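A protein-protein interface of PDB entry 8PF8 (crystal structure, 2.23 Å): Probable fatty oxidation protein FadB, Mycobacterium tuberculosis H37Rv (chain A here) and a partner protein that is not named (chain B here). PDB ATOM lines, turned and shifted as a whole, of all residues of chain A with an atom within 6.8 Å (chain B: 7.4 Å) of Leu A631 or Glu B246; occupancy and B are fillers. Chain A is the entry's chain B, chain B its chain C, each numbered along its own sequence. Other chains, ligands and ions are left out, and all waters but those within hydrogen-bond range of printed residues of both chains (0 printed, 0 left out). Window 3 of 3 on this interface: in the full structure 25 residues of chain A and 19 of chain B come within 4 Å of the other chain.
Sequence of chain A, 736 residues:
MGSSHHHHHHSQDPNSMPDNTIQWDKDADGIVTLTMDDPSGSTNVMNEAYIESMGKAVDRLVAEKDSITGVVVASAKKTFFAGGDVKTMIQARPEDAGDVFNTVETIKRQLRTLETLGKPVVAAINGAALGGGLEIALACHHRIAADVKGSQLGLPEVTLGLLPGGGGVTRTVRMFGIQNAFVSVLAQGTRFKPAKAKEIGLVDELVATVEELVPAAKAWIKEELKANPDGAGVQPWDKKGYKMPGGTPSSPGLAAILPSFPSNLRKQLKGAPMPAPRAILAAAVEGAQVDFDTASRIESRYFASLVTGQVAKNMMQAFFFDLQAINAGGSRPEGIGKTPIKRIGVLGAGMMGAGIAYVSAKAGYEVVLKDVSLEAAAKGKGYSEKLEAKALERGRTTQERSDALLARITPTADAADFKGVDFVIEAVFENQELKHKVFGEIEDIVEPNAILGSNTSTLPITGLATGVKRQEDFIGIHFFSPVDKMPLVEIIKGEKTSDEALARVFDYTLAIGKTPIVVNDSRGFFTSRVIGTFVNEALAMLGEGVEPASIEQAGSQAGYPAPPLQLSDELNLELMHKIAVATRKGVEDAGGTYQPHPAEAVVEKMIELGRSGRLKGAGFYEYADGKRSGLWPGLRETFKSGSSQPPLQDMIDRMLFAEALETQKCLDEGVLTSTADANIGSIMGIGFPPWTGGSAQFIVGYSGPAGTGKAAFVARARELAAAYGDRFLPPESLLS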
ATOM      1  N   GLU A 547      21.802 -24.414  -6.866  1.00  0.00           N
ATOM      2  CA  GLU A 547      21.823 -23.382  -5.836  1.00  0.00           C
ATOM      3  C   GLU A 547      21.197 -22.093  -6.358  1.00  0.00           C
ATOM      4  O   GLU A 547      21.496 -21.676  -7.486  1.00  0.00           O
ATOM      5  CB  GLU A 547      23.258 -23.114  -5.384  1.00  0.00           C
ATOM      6  CG  GLU A 547      23.872 -24.222  -4.550  1.00  0.00           C
ATOM      7  CD  GLU A 547      23.419 -24.185  -3.103  1.00  0.00           C
ATOM      8  OE1 GLU A 547      22.633 -23.282  -2.740  1.00  0.00           O
ATOM      9  OE2 GLU A 547      23.857 -25.058  -2.324  1.00  0.00           O
ATOM     10  N   PRO A 548      20.331 -21.435  -5.581  1.00  0.00           N
ATOM     11  CA  PRO A 548      19.732 -20.179  -6.063  1.00  0.00           C
ATOM     12  C   PRO A 548      20.758 -19.090  -6.310  1.00  0.00           C
ATOM     13  O   PRO A 548      20.574 -18.269  -7.218  1.00  0.00           O
ATOM     14  CB  PRO A 548      18.761 -19.795  -4.937  1.00  0.00           C
ATOM     15  CG  PRO A 548      18.527 -21.061  -4.174  1.00  0.00           C
ATOM     16  CD  PRO A 548      19.804 -21.833  -4.266  1.00  0.00           C
ATOM     17  N   ALA A 549      21.840 -19.060  -5.530  1.00  0.00           N
ATOM     18  CA  ALA A 549      22.883 -18.068  -5.759  1.00  0.00           C
ATOM     19  C   ALA A 549      23.536 -18.264  -7.120  1.00  0.00           C
ATOM     20  O   ALA A 549      23.862 -17.289  -7.808  1.00  0.00           O
ATOM     21  CB  ALA A 549      23.925 -18.138  -4.643  1.00  0.00           C
ATOM     22  N   SER A 550      23.727 -19.521  -7.530  1.00  0.00           N
ATOM     23  CA  SER A 550      24.336 -19.797  -8.828  1.00  0.00           C
ATOM     24  C   SER A 550      23.407 -19.427  -9.977  1.00  0.00           C
ATOM     25  O   SER A 550      23.876 -18.999 -11.038  1.00  0.00           O
ATOM     26  CB  SER A 550      24.731 -21.271  -8.921  1.00  0.00           C
ATOM     27  OG  SER A 550      25.670 -21.620  -7.919  1.00  0.00           O
ATOM     28  N   GLU A 552      21.205 -16.930  -9.957  1.00  0.00           N
ATOM     29  CA  GLU A 552      21.248 -15.478 -10.084  1.00  0.00           C
ATOM     30  C   GLU A 552      22.576 -15.011 -10.664  1.00  0.00           C
ATOM     31  O   GLU A 552      22.612 -14.062 -11.457  1.00  0.00           O
ATOM     32  CB  GLU A 552      20.988 -14.831  -8.726  1.00  0.00           C
ATOM     33  CG  GLU A 552      19.659 -15.223  -8.099  1.00  0.00           C
ATOM     34  CD  GLU A 552      18.463 -14.766  -8.913  1.00  0.00           C
ATOM     35  OE1 GLU A 552      18.163 -15.389  -9.956  1.00  0.00           O
ATOM     36  OE2 GLU A 552      17.820 -13.774  -8.512  1.00  0.00           O
ATOM     37  N   GLN A 553      23.679 -15.660 -10.282  1.00  0.00           N
ATOM     38  CA  GLN A 553      24.962 -15.332 -10.895  1.00  0.00           C
ATOM     39  C   GLN A 553      24.968 -15.691 -12.375  1.00  0.00           C
ATOM     40  O   GLN A 553      25.562 -14.975 -13.190  1.00  0.00           O
ATOM     41  CB  GLN A 553      26.099 -16.048 -10.165  1.00  0.00           C
ATOM     42  CG  GLN A 553      26.507 -15.401  -8.851  1.00  0.00           C
ATOM     43  CD  GLN A 553      27.343 -14.149  -9.047  1.00  0.00           C
ATOM     44  OE1 GLN A 553      27.675 -13.778 -10.174  1.00  0.00           O
ATOM     45  NE2 GLN A 553      27.695 -13.497  -7.945  1.00  0.00           N
ATOM     46  N   LEU A 565      15.443 -15.116 -10.858  1.00  0.00           N
ATOM     47  CA  LEU A 565      14.600 -15.280  -9.677  1.00  0.00           C
ATOM     48  C   LEU A 565      14.113 -13.931  -9.162  1.00  0.00           C
ATOM     49  O   LEU A 565      12.960 -13.803  -8.731  1.00  0.00           O
ATOM     50  CB  LEU A 565      15.348 -16.034  -8.576  1.00  0.00           C
ATOM     51  CG  LEU A 565      15.796 -17.464  -8.882  1.00  0.00           C
ATOM     52  CD1 LEU A 565      16.366 -18.132  -7.636  1.00  0.00           C
ATOM     53  CD2 LEU A 565      14.651 -18.278  -9.453  1.00  0.00           C
ATOM     54  N   GLN A 566      14.976 -12.914  -9.198  1.00  0.00           N
ATOM     55  CA  GLN A 566      14.544 -11.569  -8.836  1.00  0.00           C
ATOM     56  C   GLN A 566      13.449 -11.077  -9.773  1.00  0.00           C
ATOM     57  O   GLN A 566      12.464 -10.478  -9.330  1.00  0.00           O
ATOM     58  CB  GLN A 566      15.736 -10.614  -8.853  1.00  0.00           C
ATOM     59  CG  GLN A 566      15.364  -9.159  -8.642  1.00  0.00           C
ATOM     60  CD  GLN A 566      16.491  -8.222  -9.009  1.00  0.00           C
ATOM     61  OE1 GLN A 566      17.633  -8.409  -8.585  1.00  0.00           O
ATOM     62  NE2 GLN A 566      16.181  -7.211  -9.814  1.00  0.00           N
ATOM     63  N   ARG A 611       4.539 -17.693  -0.880  1.00  0.00           N
ATOM     64  CA  ARG A 611       5.624 -16.818  -1.323  1.00  0.00           C
ATOM     65  C   ARG A 611       5.448 -16.605  -2.823  1.00  0.00           C
ATOM     66  O   ARG A 611       6.090 -17.268  -3.639  1.00  0.00           O
ATOM     67  CB  ARG A 611       7.001 -17.417  -0.990  1.00  0.00           C
ATOM     68  CG  ARG A 611       7.389 -17.310   0.474  1.00  0.00           C
ATOM     69  CD  ARG A 611       8.834 -17.728   0.702  1.00  0.00           C
ATOM     70  NE  ARG A 611       9.392 -17.096   1.891  1.00  0.00           N
ATOM     71  CZ  ARG A 611       9.999 -15.917   1.894  1.00  0.00           C
ATOM     72  NH1 ARG A 611      10.165 -15.223   0.780  1.00  0.00           N
ATOM     73  NH2 ARG A 611      10.450 -15.419   3.042  1.00  0.00           N
ATOM     74  N   GLY A 619       8.824 -13.886  -1.770  1.00  0.00           N
ATOM     75  CA  GLY A 619       8.994 -14.723  -2.942  1.00  0.00           C
ATOM     76  C   GLY A 619      10.247 -15.567  -2.836  1.00  0.00           C
ATOM     77  O   GLY A 619      10.488 -16.195  -1.800  1.00  0.00           O
ATOM     78  N   PHE A 620      11.055 -15.602  -3.898  1.00  0.00           N
ATOM     79  CA  PHE A 620      12.360 -16.243  -3.786  1.00  0.00           C
ATOM     80  C   PHE A 620      13.294 -15.429  -2.904  1.00  0.00           C
ATOM     81  O   PHE A 620      14.206 -15.987  -2.284  1.00  0.00           O
ATOM     82  CB  PHE A 620      12.970 -16.453  -5.171  1.00  0.00           C
ATOM     83  CG  PHE A 620      12.127 -17.299  -6.078  1.00  0.00           C
ATOM     84  CD1 PHE A 620      12.040 -18.668  -5.885  1.00  0.00           C
ATOM     85  CD2 PHE A 620      11.418 -16.728  -7.121  1.00  0.00           C
ATOM     86  CE1 PHE A 620      11.259 -19.449  -6.715  1.00  0.00           C
ATOM     87  CE2 PHE A 620      10.637 -17.506  -7.955  1.00  0.00           C
ATOM     88  CZ  PHE A 620      10.557 -18.867  -7.749  1.00  0.00           C
ATOM     89  N   TYR A 621      13.075 -14.120  -2.833  1.00  0.00           N
ATOM     90  CA  TYR A 621      13.788 -13.233  -1.931  1.00  0.00           C
ATOM     91  C   TYR A 621      12.896 -12.881  -0.743  1.00  0.00           C
ATOM     92  O   TYR A 621      11.728 -13.270  -0.665  1.00  0.00           O
ATOM     93  CB  TYR A 621      14.235 -11.966  -2.661  1.00  0.00           C
ATOM     94  CG  TYR A 621      15.363 -12.171  -3.647  1.00  0.00           C
ATOM     95  CD1 TYR A 621      15.112 -12.611  -4.940  1.00  0.00           C
ATOM     96  CD2 TYR A 621      16.679 -11.912  -3.286  1.00  0.00           C
ATOM     97  CE1 TYR A 621      16.143 -12.795  -5.844  1.00  0.00           C
ATOM     98  CE2 TYR A 621      17.714 -12.090  -4.181  1.00  0.00           C
ATOM     99  CZ  TYR A 621      17.441 -12.531  -5.458  1.00  0.00           C
ATOM    100  OH  TYR A 621      18.471 -12.709  -6.351  1.00  0.00           O
ATOM    101  N   GLU A 622      13.463 -12.130   0.196  1.00  0.00           N
ATOM    102  CA  GLU A 622      12.729 -11.578   1.324  1.00  0.00           C
ATOM    103  C   GLU A 622      12.657 -10.068   1.165  1.00  0.00           C
ATOM    104  O   GLU A 622      13.666  -9.422   0.860  1.00  0.00           O
ATOM    105  CB  GLU A 622      13.390 -11.957   2.650  1.00  0.00           C
ATOM    106  CG  GLU A 622      13.433 -13.455   2.880  1.00  0.00           C
ATOM    107  CD  GLU A 622      13.236 -13.832   4.331  1.00  0.00           C
ATOM    108  OE1 GLU A 622      14.245 -13.954   5.059  1.00  0.00           O
ATOM    109  OE2 GLU A 622      12.068 -14.002   4.745  1.00  0.00           O
ATOM    110  N   ARG A 628      14.373  -5.098  -1.245  1.00  0.00           N
ATOM    111  CA  ARG A 628      14.730  -6.508  -1.275  1.00  0.00           C
ATOM    112  C   ARG A 628      16.016  -6.736  -0.492  1.00  0.00           C
ATOM    113  O   ARG A 628      16.955  -5.940  -0.577  1.00  0.00           O
ATOM    114  CB  ARG A 628      14.899  -6.973  -2.723  1.00  0.00           C
ATOM    115  CG  ARG A 628      15.581  -8.319  -2.897  1.00  0.00           C
ATOM    116  CD  ARG A 628      15.738  -8.664  -4.374  1.00  0.00           C
ATOM    117  NE  ARG A 628      16.473  -7.639  -5.109  1.00  0.00           N
ATOM    118  CZ  ARG A 628      15.919  -6.762  -5.935  1.00  0.00           C
ATOM    119  NH1 ARG A 628      14.617  -6.756  -6.166  1.00  0.00           N
ATOM    120  NH2 ARG A 628      16.692  -5.867  -6.544  1.00  0.00           N
ATOM    121  N   SER A 629      16.055  -7.828   0.277  1.00  0.00           N
ATOM    122  CA  SER A 629      17.221  -8.096   1.125  1.00  0.00           C
ATOM    123  C   SER A 629      17.368  -9.610   1.303  1.00  0.00           C
ATOM    124  O   SER A 629      16.806 -10.196   2.231  1.00  0.00           O
ATOM    125  CB  SER A 629      17.099  -7.390   2.468  1.00  0.00           C
ATOM    126  OG  SER A 629      16.092  -7.987   3.265  1.00  0.00           O
ATOM    127  N   GLY A 630      18.134 -10.223   0.412  1.00  0.00           N
ATOM    128  CA  GLY A 630      18.591 -11.594   0.603  1.00  0.00           C
ATOM    129  C   GLY A 630      17.588 -12.631   0.139  1.00  0.00           C
ATOM    130  O   GLY A 630      16.372 -12.435   0.176  1.00  0.00           O
ATOM    131  N   LEU A 631      18.120 -13.767  -0.305  1.00  0.00           N
ATOM    132  CA  LEU A 631      17.286 -14.895  -0.689  1.00  0.00           C
ATOM    133  C   LEU A 631      16.662 -15.538   0.544  1.00  0.00           C
ATOM    134  O   LEU A 631      17.243 -15.539   1.632  1.00  0.00           O
ATOM    135  CB  LEU A 631      18.108 -15.932  -1.454  1.00  0.00           C
ATOM    136  CG  LEU A 631      18.607 -15.559  -2.849  1.00  0.00           C
ATOM    137  CD1 LEU A 631      19.712 -16.507  -3.276  1.00  0.00           C
ATOM    138  CD2 LEU A 631      17.461 -15.601  -3.844  1.00  0.00           C
ATOM    139  N   TRP A 632      15.467 -16.086   0.364  1.00  0.00           N
ATOM    140  CA  TRP A 632      14.770 -16.765   1.447  1.00  0.00           C
ATOM    141  C   TRP A 632      15.580 -17.971   1.912  1.00  0.00           C
ATOM    142  O   TRP A 632      15.818 -18.890   1.116  1.00  0.00           O
ATOM    143  CB  TRP A 632      13.379 -17.195   0.983  1.00  0.00           C
ATOM    144  CG  TRP A 632      12.625 -18.027   1.976  1.00  0.00           C
ATOM    145  CD1 TRP A 632      12.450 -17.766   3.302  1.00  0.00           C
ATOM    146  CD2 TRP A 632      11.923 -19.248   1.711  1.00  0.00           C
ATOM    147  NE1 TRP A 632      11.692 -18.753   3.884  1.00  0.00           N
ATOM    148  CE2 TRP A 632      11.355 -19.675   2.928  1.00  0.00           C
ATOM    149  CE3 TRP A 632      11.724 -20.024   0.566  1.00  0.00           C
ATOM    150  CZ2 TRP A 632      10.603 -20.843   3.031  1.00  0.00           C
ATOM    151  CZ3 TRP A 632      10.975 -21.182   0.670  1.00  0.00           C
ATOM    152  CH2 TRP A 632      10.426 -21.580   1.893  1.00  0.00           C
ATOM    153  N   PRO A 633      16.030 -18.006   3.170  1.00  0.00           N
ATOM    154  CA  PRO A 633      16.887 -19.121   3.615  1.00  0.00           C
ATOM    155  C   PRO A 633      16.214 -20.483   3.558  1.00  0.00           C
ATOM    156  O   PRO A 633      16.915 -21.498   3.481  1.00  0.00           O
ATOM    157  CB  PRO A 633      17.246 -18.732   5.055  1.00  0.00           C
ATOM    158  CG  PRO A 633      17.086 -17.238   5.092  1.00  0.00           C
ATOM    159  CD  PRO A 633      15.922 -16.951   4.191  1.00  0.00           C
ATOM    160  N   GLY A 634      14.885 -20.543   3.595  1.00  0.00           N
ATOM    161  CA  GLY A 634      14.197 -21.808   3.427  1.00  0.00           C
ATOM    162  C   GLY A 634      14.192 -22.344   2.014  1.00  0.00           C
ATOM    163  O   GLY A 634      13.704 -23.456   1.789  1.00  0.00           O
ATOM    164  N   LEU A 635      14.732 -21.585   1.058  1.00  0.00           N
ATOM    165  CA  LEU A 635      14.714 -22.005  -0.338  1.00  0.00           C
ATOM    166  C   LEU A 635      15.592 -23.229  -0.572  1.00  0.00           C
ATOM    167  O   LEU A 635      15.272 -24.065  -1.423  1.00  0.00           O
ATOM    168  CB  LEU A 635      15.161 -20.844  -1.225  1.00  0.00           C
ATOM    169  CG  LEU A 635      14.681 -20.781  -2.674  1.00  0.00           C
ATOM    170  CD1 LEU A 635      13.165 -20.742  -2.736  1.00  0.00           C
ATOM    171  CD2 LEU A 635      15.273 -19.560  -3.357  1.00  0.00           C
ATOM    172  N   THR B 158      33.363 -17.934   5.408  1.00  0.00           N
ATOM    173  CA  THR B 158      31.964 -18.076   5.022  1.00  0.00           C
ATOM    174  C   THR B 158      31.665 -19.493   4.548  1.00  0.00           C
ATOM    175  O   THR B 158      30.668 -20.098   4.958  1.00  0.00           O
ATOM    176  CB  THR B 158      31.615 -17.060   3.936  1.00  0.00           C
ATOM    177  OG1 THR B 158      31.935 -15.741   4.393  1.00  0.00           O
ATOM    178  CG2 THR B 158      30.135 -17.127   3.604  1.00  0.00           C
ATOM    179  N   ASP B 235      34.334  -7.936  -3.513  1.00  0.00           N
ATOM    180  CA  ASP B 235      33.318  -8.904  -3.106  1.00  0.00           C
ATOM    181  C   ASP B 235      32.586  -9.464  -4.318  1.00  0.00           C
ATOM    182  O   ASP B 235      32.397 -10.679  -4.438  1.00  0.00           O
ATOM    183  CB  ASP B 235      32.326  -8.261  -2.135  1.00  0.00           C
ATOM    184  CG  ASP B 235      32.688  -8.504  -0.685  1.00  0.00           C
ATOM    185  OD1 ASP B 235      33.829  -8.934  -0.420  1.00  0.00           O
ATOM    186  OD2 ASP B 235      31.826  -8.276   0.192  1.00  0.00           O
ATOM    187  N   LEU B 239      32.575 -13.431  -5.690  1.00  0.00           N
ATOM    188  CA  LEU B 239      31.353 -14.214  -5.825  1.00  0.00           C
ATOM    189  C   LEU B 239      31.038 -14.580  -7.270  1.00  0.00           C
ATOM    190  O   LEU B 239      30.235 -15.489  -7.497  1.00  0.00           O
ATOM    191  CB  LEU B 239      30.177 -13.455  -5.206  1.00  0.00           C
ATOM    192  CG  LEU B 239      30.291 -13.220  -3.696  1.00  0.00           C
ATOM    193  CD1 LEU B 239      29.025 -12.586  -3.145  1.00  0.00           C
ATOM    194  CD2 LEU B 239      30.607 -14.517  -2.966  1.00  0.00           C
ATOM    195  N   TYR B 242      32.982 -17.900  -7.088  1.00  0.00           N
ATOM    196  CA  TYR B 242      32.301 -18.729  -6.090  1.00  0.00           C
ATOM    197  C   TYR B 242      30.811 -18.386  -6.093  1.00  0.00           C
ATOM    198  O   TYR B 242      30.253 -17.825  -5.148  1.00  0.00           O
ATOM    199  CB  TYR B 242      32.938 -18.534  -4.720  1.00  0.00           C
ATOM    200  CG  TYR B 242      34.353 -19.067  -4.653  1.00  0.00           C
ATOM    201  CD1 TYR B 242      35.434 -18.287  -5.049  1.00  0.00           C
ATOM    202  CD2 TYR B 242      34.604 -20.358  -4.215  1.00  0.00           C
ATOM    203  CE1 TYR B 242      36.727 -18.780  -5.001  1.00  0.00           C
ATOM    204  CE2 TYR B 242      35.889 -20.859  -4.163  1.00  0.00           C
ATOM    205  CZ  TYR B 242      36.947 -20.069  -4.557  1.00  0.00           C
ATOM    206  OH  TYR B 242      38.224 -20.578  -4.501  1.00  0.00           O
ATOM    207  N   HIS B 243      30.162 -18.757  -7.202  1.00  0.00           N
ATOM    208  CA  HIS B 243      28.805 -18.300  -7.483  1.00  0.00           C
ATOM    209  C   HIS B 243      27.756 -18.948  -6.591  1.00  0.00           C
ATOM    210  O   HIS B 243      26.650 -18.409  -6.477  1.00  0.00           O
ATOM    211  CB  HIS B 243      28.460 -18.545  -8.953  1.00  0.00           C
ATOM    212  CG  HIS B 243      28.819 -19.914  -9.442  1.00  0.00           C
ATOM    213  ND1 HIS B 243      28.041 -21.025  -9.190  1.00  0.00           N
ATOM    214  CD2 HIS B 243      29.869 -20.350 -10.176  1.00  0.00           C
ATOM    215  CE1 HIS B 243      28.599 -22.085  -9.746  1.00  0.00           C
ATOM    216  NE2 HIS B 243      29.709 -21.703 -10.350  1.00  0.00           N
ATOM    217  N   TRP B 244      28.063 -20.083  -5.963  1.00  0.00           N
ATOM    218  CA  TRP B 244      27.111 -20.700  -5.047  1.00  0.00           C
ATOM    219  C   TRP B 244      27.031 -19.984  -3.705  1.00  0.00           C
ATOM    220  O   TRP B 244      26.154 -20.314  -2.899  1.00  0.00           O
ATOM    221  CB  TRP B 244      27.460 -22.174  -4.821  1.00  0.00           C
ATOM    222  CG  TRP B 244      28.843 -22.400  -4.300  1.00  0.00           C
ATOM    223  CD1 TRP B 244      29.219 -22.523  -2.992  1.00  0.00           C
ATOM    224  CD2 TRP B 244      30.038 -22.535  -5.076  1.00  0.00           C
ATOM    225  NE1 TRP B 244      30.576 -22.725  -2.908  1.00  0.00           N
ATOM    226  CE2 TRP B 244      31.102 -22.736  -4.173  1.00  0.00           C
ATOM    227  CE3 TRP B 244      30.313 -22.502  -6.446  1.00  0.00           C
ATOM    228  CZ2 TRP B 244      32.418 -22.906  -4.599  1.00  0.00           C
ATOM    229  CZ3 TRP B 244      31.620 -22.671  -6.866  1.00  0.00           C
ATOM    230  CH2 TRP B 244      32.655 -22.869  -5.945  1.00  0.00           C
ATOM    231  N   VAL B 245      27.913 -19.019  -3.448  1.00  0.00           N
ATOM    232  CA  VAL B 245      27.912 -18.243  -2.211  1.00  0.00           C
ATOM    233  C   VAL B 245      27.188 -16.930  -2.466  1.00  0.00           C
ATOM    234  O   VAL B 245      27.528 -16.194  -3.401  1.00  0.00           O
ATOM    235  CB  VAL B 245      29.345 -17.993  -1.711  1.00  0.00           C
ATOM    236  CG1 VAL B 245      29.328 -17.178  -0.425  1.00  0.00           C
ATOM    237  CG2 VAL B 245      30.066 -19.311  -1.507  1.00  0.00           C
ATOM    238  N   GLU B 246      26.194 -16.628  -1.630  1.00  0.00           N
ATOM    239  CA  GLU B 246      25.372 -15.444  -1.853  1.00  0.00           C
ATOM    240  C   GLU B 246      26.035 -14.180  -1.319  1.00  0.00           C
ATOM    241  O   GLU B 246      25.969 -13.124  -1.959  1.00  0.00           O
ATOM    242  CB  GLU B 246      24.001 -15.628  -1.205  1.00  0.00           C
ATOM    243  CG  GLU B 246      23.087 -14.423  -1.351  1.00  0.00           C
ATOM    244  CD  GLU B 246      21.785 -14.587  -0.595  1.00  0.00           C
ATOM    245  OE1 GLU B 246      21.637 -15.601   0.121  1.00  0.00           O
ATOM    246  OE2 GLU B 246      20.913 -13.702  -0.717  1.00  0.00           O
ATOM    247  N   LYS B 247      26.676 -14.266  -0.156  1.00  0.00           N
ATOM    248  CA  LYS B 247      27.194 -13.089   0.525  1.00  0.00           C
ATOM    249  C   LYS B 247      28.400 -13.483   1.368  1.00  0.00           C
ATOM    250  O   LYS B 247      28.395 -14.533   2.019  1.00  0.00           O
ATOM    251  CB  LYS B 247      26.108 -12.450   1.401  1.00  0.00           C
ATOM    252  CG  LYS B 247      26.407 -11.038   1.871  1.00  0.00           C
ATOM    253  CD  LYS B 247      25.205 -10.456   2.605  1.00  0.00           C
ATOM    254  CE  LYS B 247      25.401  -8.984   2.932  1.00  0.00           C
ATOM    255  NZ  LYS B 247      26.521  -8.763   3.887  1.00  0.00           N
ATOM    256  N   ILE B 248      29.427 -12.639   1.351  1.00  0.00           N
ATOM    257  CA  ILE B 248      30.651 -12.884   2.105  1.00  0.00           C
ATOM    258  C   ILE B 248      30.499 -12.301   3.503  1.00  0.00           C
ATOM    259  O   ILE B 248      30.189 -11.114   3.662  1.00  0.00           O
ATOM    260  CB  ILE B 248      31.871 -12.280   1.388  1.00  0.00           C
ATOM    261  CG1 ILE B 248      32.148 -13.025   0.081  1.00  0.00           C
ATOM    262  CG2 ILE B 248      33.091 -12.317   2.291  1.00  0.00           C
ATOM    263  CD1 ILE B 248      33.310 -12.458  -0.706  1.00  0.00           C
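The backbone carbonyl oxygen (O) of Gly A630 lies within hydrogen-bond range of the backbone NH (N) of Glu A622.
Along chain B the printed residues that touch a printed residue of chain A span positions 239 to 246.
Among the printed residues, 8 pairs touch across the chains.
The side-chain hydroxyl (OG) of Ser A550 lies close to the backbone NH (N) of Trp B244 (3.5 Å).
The backbone carbonyl oxygen (O) of Ala A549 lies close to the backbone carbonyl oxygen (O) of His B243 (3.3 Å).
The side-chain hydroxyl (OG) of Ser A550 sits at hydrogen-bond distance from a ring nitrogen (ND1) of His B243 (2.8 Å).
The backbone carbonyl oxygen of Leu B239 lies within hydrogen-bond range of the side-chain amide nitrogen of Gln A553.
The backbone NH (N) of Leu A631 lies within hydrogen-bond range of the side-chain carboxylate (OE2) of Glu B246 (2.8 Å).
Of chain A, only Gly A630 and Leu A631 come within 4 Å of Glu B246.
Of the printed residues of chain A, Trp B244 touches Ala A549 and Ser A550.
Printed residues of chain B within 4 Å of Gly A630: Glu B246.
Printed residues of chain A within 4 Å of His B243: Ala A549 (3.2 Å), Ser A550 (2.8 Å) and Gln A553 (3.6 Å).
Of the printed residues of chain B, Ser A550 touches His B243 and Trp B244.
The nearest residue of chain A that does not touch Glu B246 is Ala A549 (4.1 Å).
Trp B244 touches Ala A549 (O to CB, 3.6 Å).
CB of Gln A553 touches CB of His B243 (3.6 Å).
OE2 of Glu B246 touches CA of Gly A630 (3.4 Å).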
